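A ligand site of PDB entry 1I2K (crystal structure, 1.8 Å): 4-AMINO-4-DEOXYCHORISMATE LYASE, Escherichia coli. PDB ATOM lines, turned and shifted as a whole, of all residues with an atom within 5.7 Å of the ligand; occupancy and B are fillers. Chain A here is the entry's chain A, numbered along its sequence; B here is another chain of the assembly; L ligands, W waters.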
ATOM      1  N   PHE A  26     -20.897  -1.335  19.215  1.00  0.00           N
ATOM      2  CA  PHE A  26     -19.638  -0.997  19.909  1.00  0.00           C
ATOM      3  C   PHE A  26     -19.351  -1.996  21.038  1.00  0.00           C
ATOM      4  O   PHE A  26     -20.246  -2.771  21.363  1.00  0.00           O
ATOM      5  CB  PHE A  26     -19.691   0.433  20.428  1.00  0.00           C
ATOM      6  CG  PHE A  26     -20.640   0.739  21.582  1.00  0.00           C
ATOM      7  CD1 PHE A  26     -22.009   0.829  21.393  1.00  0.00           C
ATOM      8  CD2 PHE A  26     -20.143   0.960  22.859  1.00  0.00           C
ATOM      9  CE1 PHE A  26     -22.855   1.135  22.446  1.00  0.00           C
ATOM     10  CE2 PHE A  26     -20.977   1.260  23.930  1.00  0.00           C
ATOM     11  CZ  PHE A  26     -22.337   1.342  23.721  1.00  0.00           C
ATOM     12  N   THR A  27     -18.132  -1.941  21.582  1.00  0.00           N
ATOM     13  CA  THR A  27     -17.861  -2.668  22.833  1.00  0.00           C
ATOM     14  C   THR A  27     -16.950  -1.825  23.717  1.00  0.00           C
ATOM     15  O   THR A  27     -16.199  -0.982  23.204  1.00  0.00           O
ATOM     16  CB  THR A  27     -17.265  -4.061  22.543  1.00  0.00           C
ATOM     17  OG1 THR A  27     -17.454  -4.933  23.670  1.00  0.00           O
ATOM     18  CG2 THR A  27     -15.753  -3.987  22.309  1.00  0.00           C
ATOM     19  N   THR A  28     -16.991  -2.033  25.032  1.00  0.00           N
ATOM     20  CA  THR A  28     -15.987  -1.415  25.895  1.00  0.00           C
ATOM     21  C   THR A  28     -15.336  -2.520  26.737  1.00  0.00           C
ATOM     22  O   THR A  28     -16.018  -3.306  27.430  1.00  0.00           O
ATOM     23  CB  THR A  28     -16.559  -0.299  26.791  1.00  0.00           C
ATOM     24  OG1 THR A  28     -17.689  -0.787  27.516  1.00  0.00           O
ATOM     25  CG2 THR A  28     -17.097   0.848  25.954  1.00  0.00           C
ATOM     26  N   HIS A  42     -15.109 -10.288  23.246  1.00  0.00           N
ATOM     27  CA  HIS A  42     -15.374  -8.959  22.682  1.00  0.00           C
ATOM     28  C   HIS A  42     -15.410  -9.071  21.169  1.00  0.00           C
ATOM     29  O   HIS A  42     -16.243  -8.467  20.503  1.00  0.00           O
ATOM     30  CB  HIS A  42     -14.303  -7.973  23.158  1.00  0.00           C
ATOM     31  CG  HIS A  42     -14.582  -7.445  24.538  1.00  0.00           C
ATOM     32  ND1 HIS A  42     -15.585  -6.525  24.774  1.00  0.00           N
ATOM     33  CD2 HIS A  42     -14.022  -7.689  25.750  1.00  0.00           C
ATOM     34  CE1 HIS A  42     -15.623  -6.225  26.073  1.00  0.00           C
ATOM     35  NE2 HIS A  42     -14.677  -6.923  26.682  1.00  0.00           N
ATOM     36  N   ARG A  45     -18.710 -10.739  20.316  1.00  0.00           N
ATOM     37  CA  ARG A  45     -19.919  -9.919  20.454  1.00  0.00           C
ATOM     38  C   ARG A  45     -20.017  -8.918  19.309  1.00  0.00           C
ATOM     39  O   ARG A  45     -21.124  -8.627  18.792  1.00  0.00           O
ATOM     40  CB  ARG A  45     -19.935  -9.214  21.824  1.00  0.00           C
ATOM     41  CG  ARG A  45     -19.149  -7.919  21.923  1.00  0.00           C
ATOM     42  CD  ARG A  45     -19.985  -6.659  21.965  1.00  0.00           C
ATOM     43  NE  ARG A  45     -21.067  -6.746  22.952  1.00  0.00           N
ATOM     44  CZ  ARG A  45     -20.964  -6.375  24.221  1.00  0.00           C
ATOM     45  NH1 ARG A  45     -19.826  -5.871  24.706  1.00  0.00           N
ATOM     46  NH2 ARG A  45     -22.028  -6.514  25.011  1.00  0.00           N
ATOM     47  N   LYS A 140     -25.243  -4.769  21.486  1.00  0.00           N
ATOM     48  CA  LYS A 140     -24.771  -3.457  21.962  1.00  0.00           C
ATOM     49  C   LYS A 140     -24.648  -2.465  20.809  1.00  0.00           C
ATOM     50  O   LYS A 140     -23.531  -2.097  20.411  1.00  0.00           O
ATOM     51  CB  LYS A 140     -23.404  -3.636  22.630  1.00  0.00           C
ATOM     52  CG  LYS A 140     -22.989  -2.540  23.604  1.00  0.00           C
ATOM     53  CD  LYS A 140     -21.826  -3.012  24.468  1.00  0.00           C
ATOM     54  CE  LYS A 140     -21.340  -1.995  25.475  1.00  0.00           C
ATOM     55  NZ  LYS A 140     -22.382  -1.557  26.445  1.00  0.00           N
ATOM     56  N   ARG A 144     -28.358   4.721  21.504  1.00  0.00           N
ATOM     57  CA  ARG A 144     -28.439   4.633  22.967  1.00  0.00           C
ATOM     58  C   ARG A 144     -29.074   5.846  23.616  1.00  0.00           C
ATOM     59  O   ARG A 144     -28.742   6.176  24.764  1.00  0.00           O
ATOM     60  CB  ARG A 144     -27.012   4.396  23.528  1.00  0.00           C
ATOM     61  CG  ARG A 144     -26.358   3.186  22.901  1.00  0.00           C
ATOM     62  CD  ARG A 144     -26.513   1.893  23.642  1.00  0.00           C
ATOM     63  NE  ARG A 144     -27.811   1.285  23.848  1.00  0.00           N
ATOM     64  CZ  ARG A 144     -28.232   0.101  23.401  1.00  0.00           C
ATOM     65  NH1 ARG A 144     -27.472  -0.700  22.668  1.00  0.00           N
ATOM     66  NH2 ARG A 144     -29.461  -0.316  23.700  1.00  0.00           N
ATOM     67  N   GLN A 147     -30.637   5.152  26.995  1.00  0.00           N
ATOM     68  CA  GLN A 147     -29.685   5.164  28.086  1.00  0.00           C
ATOM     69  C   GLN A 147     -29.271   6.587  28.431  1.00  0.00           C
ATOM     70  O   GLN A 147     -29.035   6.908  29.598  1.00  0.00           O
ATOM     71  CB  GLN A 147     -28.431   4.340  27.764  1.00  0.00           C
ATOM     72  CG  GLN A 147     -28.682   2.825  27.824  1.00  0.00           C
ATOM     73  CD  GLN A 147     -29.637   2.347  26.743  1.00  0.00           C
ATOM     74  OE1 GLN A 147     -29.562   2.734  25.568  1.00  0.00           O
ATOM     75  NE2 GLN A 147     -30.570   1.516  27.161  1.00  0.00           N
ATOM     76  N   GLU A 173     -32.845  -4.388  33.024  1.00  0.00           N
ATOM     77  CA  GLU A 173     -31.431  -4.122  33.271  1.00  0.00           C
ATOM     78  C   GLU A 173     -31.204  -2.850  34.067  1.00  0.00           C
ATOM     79  O   GLU A 173     -32.118  -2.268  34.666  1.00  0.00           O
ATOM     80  CB  GLU A 173     -30.670  -4.066  31.924  1.00  0.00           C
ATOM     81  CG  GLU A 173     -30.938  -2.883  31.020  1.00  0.00           C
ATOM     82  CD  GLU A 173     -30.186  -2.878  29.698  1.00  0.00           C
ATOM     83  OE1 GLU A 173     -29.254  -3.676  29.485  1.00  0.00           O
ATOM     84  OE2 GLU A 173     -30.529  -2.076  28.779  1.00  0.00           O
ATOM     85  N   CYS A 174     -29.948  -2.377  34.100  1.00  0.00           N
ATOM     86  CA  CYS A 174     -29.605  -1.063  34.650  1.00  0.00           C
ATOM     87  C   CYS A 174     -29.311  -0.053  33.545  1.00  0.00           C
ATOM     88  O   CYS A 174     -29.712  -0.263  32.396  1.00  0.00           O
ATOM     89  CB  CYS A 174     -28.381  -1.117  35.576  1.00  0.00           C
ATOM     90  SG  CYS A 174     -28.621  -2.382  36.871  1.00  0.00           S
ATOM     91  N   CYS A 175     -28.618   1.043  33.855  1.00  0.00           N
ATOM     92  CA  CYS A 175     -28.353   2.040  32.809  1.00  0.00           C
ATOM     93  C   CYS A 175     -27.203   1.559  31.921  1.00  0.00           C
ATOM     94  O   CYS A 175     -27.285   1.611  30.685  1.00  0.00           O
ATOM     95  CB  CYS A 175     -28.000   3.429  33.366  1.00  0.00           C
ATOM     96  SG  CYS A 175     -27.821   4.702  32.053  1.00  0.00           S
ATOM     97  N   ALA A 176     -26.127   1.058  32.519  1.00  0.00           N
ATOM     98  CA  ALA A 176     -24.986   0.621  31.723  1.00  0.00           C
ATOM     99  C   ALA A 176     -24.404  -0.709  32.197  1.00  0.00           C
ATOM    100  O   ALA A 176     -23.228  -1.012  31.973  1.00  0.00           O
ATOM    101  CB  ALA A 176     -23.902   1.695  31.745  1.00  0.00           C
ATOM    102  N   ALA A 177     -25.264  -1.458  32.865  1.00  0.00           N
ATOM    103  CA  ALA A 177     -24.909  -2.723  33.492  1.00  0.00           C
ATOM    104  C   ALA A 177     -26.087  -3.702  33.462  1.00  0.00           C
ATOM    105  O   ALA A 177     -27.209  -3.246  33.271  1.00  0.00           O
ATOM    106  CB  ALA A 177     -24.513  -2.495  34.940  1.00  0.00           C
ATOM    107  N   ASN A 178     -25.797  -4.994  33.674  1.00  0.00           N
ATOM    108  CA  ASN A 178     -26.853  -6.001  33.750  1.00  0.00           C
ATOM    109  C   ASN A 178     -27.140  -6.322  35.227  1.00  0.00           C
ATOM    110  O   ASN A 178     -26.328  -5.938  36.080  1.00  0.00           O
ATOM    111  CB  ASN A 178     -26.500  -7.269  32.970  1.00  0.00           C
ATOM    112  CG  ASN A 178     -26.550  -7.023  31.465  1.00  0.00           C
ATOM    113  OD1 ASN A 178     -25.516  -7.116  30.787  1.00  0.00           O
ATOM    114  ND2 ASN A 178     -27.736  -6.680  30.948  1.00  0.00           N
ATOM    115  N   VAL A 197     -29.197  -4.987  26.707  1.00  0.00           N
ATOM    116  CA  VAL A 197     -27.925  -5.417  26.115  1.00  0.00           C
ATOM    117  C   VAL A 197     -27.449  -6.703  26.795  1.00  0.00           C
ATOM    118  O   VAL A 197     -27.368  -6.721  28.017  1.00  0.00           O
ATOM    119  CB  VAL A 197     -26.795  -4.393  26.262  1.00  0.00           C
ATOM    120  CG1 VAL A 197     -25.445  -4.993  25.884  1.00  0.00           C
ATOM    121  CG2 VAL A 197     -27.046  -3.136  25.440  1.00  0.00           C
ATOM    122  N   ASN A 198     -27.176  -7.739  25.993  1.00  0.00           N
ATOM    123  CA  ASN A 198     -26.767  -9.030  26.539  1.00  0.00           C
ATOM    124  C   ASN A 198     -25.282  -8.977  26.845  1.00  0.00           C
ATOM    125  O   ASN A 198     -24.445  -9.394  26.025  1.00  0.00           O
ATOM    126  CB  ASN A 198     -27.115 -10.154  25.572  1.00  0.00           C
ATOM    127  CG  ASN A 198     -26.664 -11.516  26.097  1.00  0.00           C
ATOM    128  OD1 ASN A 198     -26.219 -11.658  27.233  1.00  0.00           O
ATOM    129  ND2 ASN A 198     -26.787 -12.507  25.228  1.00  0.00           N
ATOM    130  N   GLY A 199     -24.918  -8.412  28.004  1.00  0.00           N
ATOM    131  CA  GLY A 199     -23.522  -8.016  28.180  1.00  0.00           C
ATOM    132  C   GLY A 199     -22.532  -9.169  28.181  1.00  0.00           C
ATOM    133  O   GLY A 199     -22.881 -10.315  28.465  1.00  0.00           O
ATOM    134  N   ILE A 200     -21.265  -8.845  27.876  1.00  0.00           N
ATOM    135  CA  ILE A 200     -20.156  -9.797  27.987  1.00  0.00           C
ATOM    136  C   ILE A 200     -20.013 -10.310  29.391  1.00  0.00           C
ATOM    137  O   ILE A 200     -19.748 -11.498  29.651  1.00  0.00           O
ATOM    138  CB  ILE A 200     -18.853  -9.103  27.480  1.00  0.00           C
ATOM    139  CG1 ILE A 200     -18.310  -9.807  26.228  1.00  0.00           C
ATOM    140  CG2 ILE A 200     -17.753  -8.944  28.511  1.00  0.00           C
ATOM    141  CD1 ILE A 200     -19.126  -9.508  25.004  1.00  0.00           C
ATOM    142  N   MET A 201     -20.176  -9.426  30.393  1.00  0.00           N
ATOM    143  CA  MET A 201     -19.983  -9.917  31.768  1.00  0.00           C
ATOM    144  C   MET A 201     -21.195 -10.737  32.181  1.00  0.00           C
ATOM    145  O   MET A 201     -21.028 -11.745  32.906  1.00  0.00           O
ATOM    146  CB  MET A 201     -19.665  -8.789  32.757  1.00  0.00           C
ATOM    147  CG  MET A 201     -19.182  -9.264  34.117  1.00  0.00           C
ATOM    148  SD  MET A 201     -17.687 -10.245  34.121  1.00  0.00           S
ATOM    149  CE  MET A 201     -16.538  -9.186  33.219  1.00  0.00           C
ATOM    150  N   ARG A 202     -22.378 -10.342  31.711  1.00  0.00           N
ATOM    151  CA  ARG A 202     -23.584 -11.147  32.013  1.00  0.00           C
ATOM    152  C   ARG A 202     -23.383 -12.581  31.521  1.00  0.00           C
ATOM    153  O   ARG A 202     -23.633 -13.563  32.219  1.00  0.00           O
ATOM    154  CB  ARG A 202     -24.827 -10.530  31.380  1.00  0.00           C
ATOM    155  CG  ARG A 202     -26.088 -11.403  31.408  1.00  0.00           C
ATOM    156  CD  ARG A 202     -27.154 -10.794  30.491  1.00  0.00           C
ATOM    157  NE  ARG A 202     -28.441 -11.468  30.634  1.00  0.00           N
ATOM    158  CZ  ARG A 202     -28.884 -12.514  29.947  1.00  0.00           C
ATOM    159  NH1 ARG A 202     -28.164 -13.080  29.001  1.00  0.00           N
ATOM    160  NH2 ARG A 202     -30.085 -13.036  30.174  1.00  0.00           N
ATOM    161  N   CYS A 235     -23.424  -5.894  36.914  1.00  0.00           N
ATOM    162  CA  CYS A 235     -22.157  -6.213  36.252  1.00  0.00           C
ATOM    163  C   CYS A 235     -22.000  -5.585  34.872  1.00  0.00           C
ATOM    164  O   CYS A 235     -22.973  -5.271  34.186  1.00  0.00           O
ATOM    165  CB  CYS A 235     -22.038  -7.738  36.103  1.00  0.00           C
ATOM    166  SG  CYS A 235     -23.298  -8.464  34.987  1.00  0.00           S
ATOM    167  N   ASN A 236     -20.750  -5.401  34.459  1.00  0.00           N
ATOM    168  CA  ASN A 236     -20.459  -4.992  33.077  1.00  0.00           C
ATOM    169  C   ASN A 236     -18.978  -5.305  32.808  1.00  0.00           C
ATOM    170  O   ASN A 236     -18.294  -5.765  33.743  1.00  0.00           O
ATOM    171  CB  ASN A 236     -20.842  -3.547  32.790  1.00  0.00           C
ATOM    172  CG  ASN A 236     -20.026  -2.474  33.441  1.00  0.00           C
ATOM    173  OD1 ASN A 236     -18.905  -2.716  33.883  1.00  0.00           O
ATOM    174  ND2 ASN A 236     -20.615  -1.273  33.524  1.00  0.00           N
ATOM    175  N   ALA A 237     -18.485  -5.126  31.596  1.00  0.00           N
ATOM    176  CA  ALA A 237     -17.098  -5.558  31.380  1.00  0.00           C
ATOM    177  C   ALA A 237     -16.110  -4.827  32.270  1.00  0.00           C
ATOM    178  O   ALA A 237     -15.008  -5.290  32.579  1.00  0.00           O
ATOM    179  CB  ALA A 237     -16.725  -5.338  29.914  1.00  0.00           C
ATOM    180  N   LEU A 238     -16.478  -3.633  32.719  1.00  0.00           N
ATOM    181  CA  LEU A 238     -15.486  -2.783  33.372  1.00  0.00           C
ATOM    182  C   LEU A 238     -15.478  -2.819  34.883  1.00  0.00           C
ATOM    183  O   LEU A 238     -14.436  -2.556  35.487  1.00  0.00           O
ATOM    184  CB  LEU A 238     -15.767  -1.333  32.930  1.00  0.00           C
ATOM    185  CG  LEU A 238     -15.717  -1.084  31.434  1.00  0.00           C
ATOM    186  CD1 LEU A 238     -15.835   0.410  31.144  1.00  0.00           C
ATOM    187  CD2 LEU A 238     -14.452  -1.641  30.800  1.00  0.00           C
ATOM    188  N   TYR B  92     -22.728   7.538  29.484  1.00  0.00           N
ATOM    189  CA  TYR B  92     -23.938   8.116  28.903  1.00  0.00           C
ATOM    190  C   TYR B  92     -24.285   9.468  29.521  1.00  0.00           C
ATOM    191  O   TYR B  92     -25.231  10.115  29.048  1.00  0.00           O
ATOM    192  CB  TYR B  92     -25.126   7.148  29.065  1.00  0.00           C
ATOM    193  CG  TYR B  92     -24.968   5.822  28.355  1.00  0.00           C
ATOM    194  CD1 TYR B  92     -24.684   5.743  27.002  1.00  0.00           C
ATOM    195  CD2 TYR B  92     -25.092   4.610  29.048  1.00  0.00           C
ATOM    196  CE1 TYR B  92     -24.548   4.514  26.369  1.00  0.00           C
ATOM    197  CE2 TYR B  92     -24.942   3.380  28.417  1.00  0.00           C
ATOM    198  CZ  TYR B  92     -24.668   3.343  27.069  1.00  0.00           C
ATOM    199  OH  TYR B  92     -24.521   2.137  26.433  1.00  0.00           O
HETATM  200  N1  LIG L   1     -26.362  -2.642  29.530  1.00  0.00           N
HETATM  201  C1  LIG L   1     -26.215  -1.631  28.600  1.00  0.00           C
HETATM  202  C2  LIG L   1     -27.380  -0.750  28.293  1.00  0.00           C
HETATM  203  C3  LIG L   1     -24.953  -1.556  28.044  1.00  0.00           C
HETATM  204  O1  LIG L   1     -24.738  -0.484  27.179  1.00  0.00           O
HETATM  205  C4  LIG L   1     -23.899  -2.391  28.381  1.00  0.00           C
HETATM  206  C5  LIG L   1     -22.624  -2.229  27.597  1.00  0.00           C
HETATM  207  C6  LIG L   1     -24.149  -3.404  29.326  1.00  0.00           C
HETATM  208  C7  LIG L   1     -25.387  -3.540  29.915  1.00  0.00           C
HETATM  209  C8  LIG L   1     -23.087  -4.312  29.842  1.00  0.00           C
HETATM  210  O2  LIG L   1     -22.357  -4.889  28.705  1.00  0.00           O
HETATM  211  P1  LIG L   1     -21.009  -5.675  28.964  1.00  0.00           P
HETATM  212  O3  LIG L   1     -20.136  -4.517  29.289  1.00  0.00           O
HETATM  213  O4  LIG L   1     -20.741  -6.306  27.623  1.00  0.00           O
HETATM  214  O5  LIG L   1     -21.003  -6.634  30.091  1.00  0.00           O
HETATM  215  O   HOH W   1     -22.974  -7.572  31.661  1.00  0.00           O
HETATM  216  O   HOH W   2     -19.314  -1.978  29.445  1.00  0.00           O
HETATM  217  O   HOH W   3     -18.593  -3.981  26.939  1.00  0.00           O
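The backbone NH of Phe 26 lies within hydrogen-bond range of the backbone carbonyl oxygen of Lys 140, 3.0 Å away.
The guanidinium group (NH1) of Arg 45 sits at hydrogen-bond distance from the side-chain hydroxyl (OG1) of Thr 27 (2.8 Å).
OE1 of Glu 173 lies within hydrogen-bond range of N of Val 197 (3.1 Å).
The backbone NH (N) of Gly 199 is in hydrogen-bond range of the side-chain amide oxygen (OD1) of Asn 178.
ND2 of Asn 236 is in hydrogen-bond range of O of Ala 176, 3.0 Å away.
The backbone NH (N) of Leu 238 lies within hydrogen-bond range of the side-chain amide oxygen (OD1) of Asn 236, at 2.8 Å.
N of Asn 178 sits at hydrogen-bond distance from O of Cys 235 (2.9 Å).
The side-chain amide oxygen (OE1) of Gln 147 sits at hydrogen-bond distance from the guanidinium group (NE) of Arg 144.
Water W2 bridges O3 of the ligand (2.7 Å) and OG1 of Thr 28 (2.8 Å).
Water W1 lies within hydrogen-bond range of an oxygen (O5) of the ligand (2.7 Å), the side-chain amide oxygen of Asn 178 (2.7 Å), the backbone NH of Arg 202 (2.8 Å) and the backbone carbonyl oxygen of Cys 235 (3.4 Å).
Water W3 lies within hydrogen-bond range of O of Thr 28, O3 of the ligand and NH1 of Arg 45.
NZ of Lys 140 is bonded to C5 of the ligand.
An oxygen (O4) of the ligand lies within hydrogen-bond range of the backbone NH of Ile 200, at 2.6 Å.
The side-chain hydroxyl (OH) of Tyr 92 of chain B is in hydrogen-bond range of an oxygen (O1) of the ligand.
The backbone NH (N) of Ala 237 sits at hydrogen-bond distance from an oxygen (O3) of the ligand, 2.9 Å away.
O4 of the ligand lies within salt-bridge range of NH2 of Arg 45 (2.9 Å).
O5 of the ligand lies within hydrogen-bond range of N of Met 201, 2.9 Å away.
A nitrogen (N1) of the ligand sits close to the side-chain carboxylate (OE1) of Glu 173, at 3.1 Å.
Gln 147 touches the ligand (CG to C2, 3.8 Å).
Cys 175 touches the ligand.
O of Ala 176 touches C6 of the ligand (3.7 Å).
Ala 177 touches the ligand.
Asn 178 touches the ligand.
Val 197 touches the ligand.
Gly 199 touches the ligand (CA to O4, 3.3 Å).
CA of Asn 236 touches O5 of the ligand (3.5 Å).
Hydrophobic or aromatic side chains that line the ligand: Val 197, Ile 200, Met 201, Ala 237 and Tyr 92 of chain B.
The nearest printed residue that does not touch the ligand is Arg 202 (4.3 Å).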
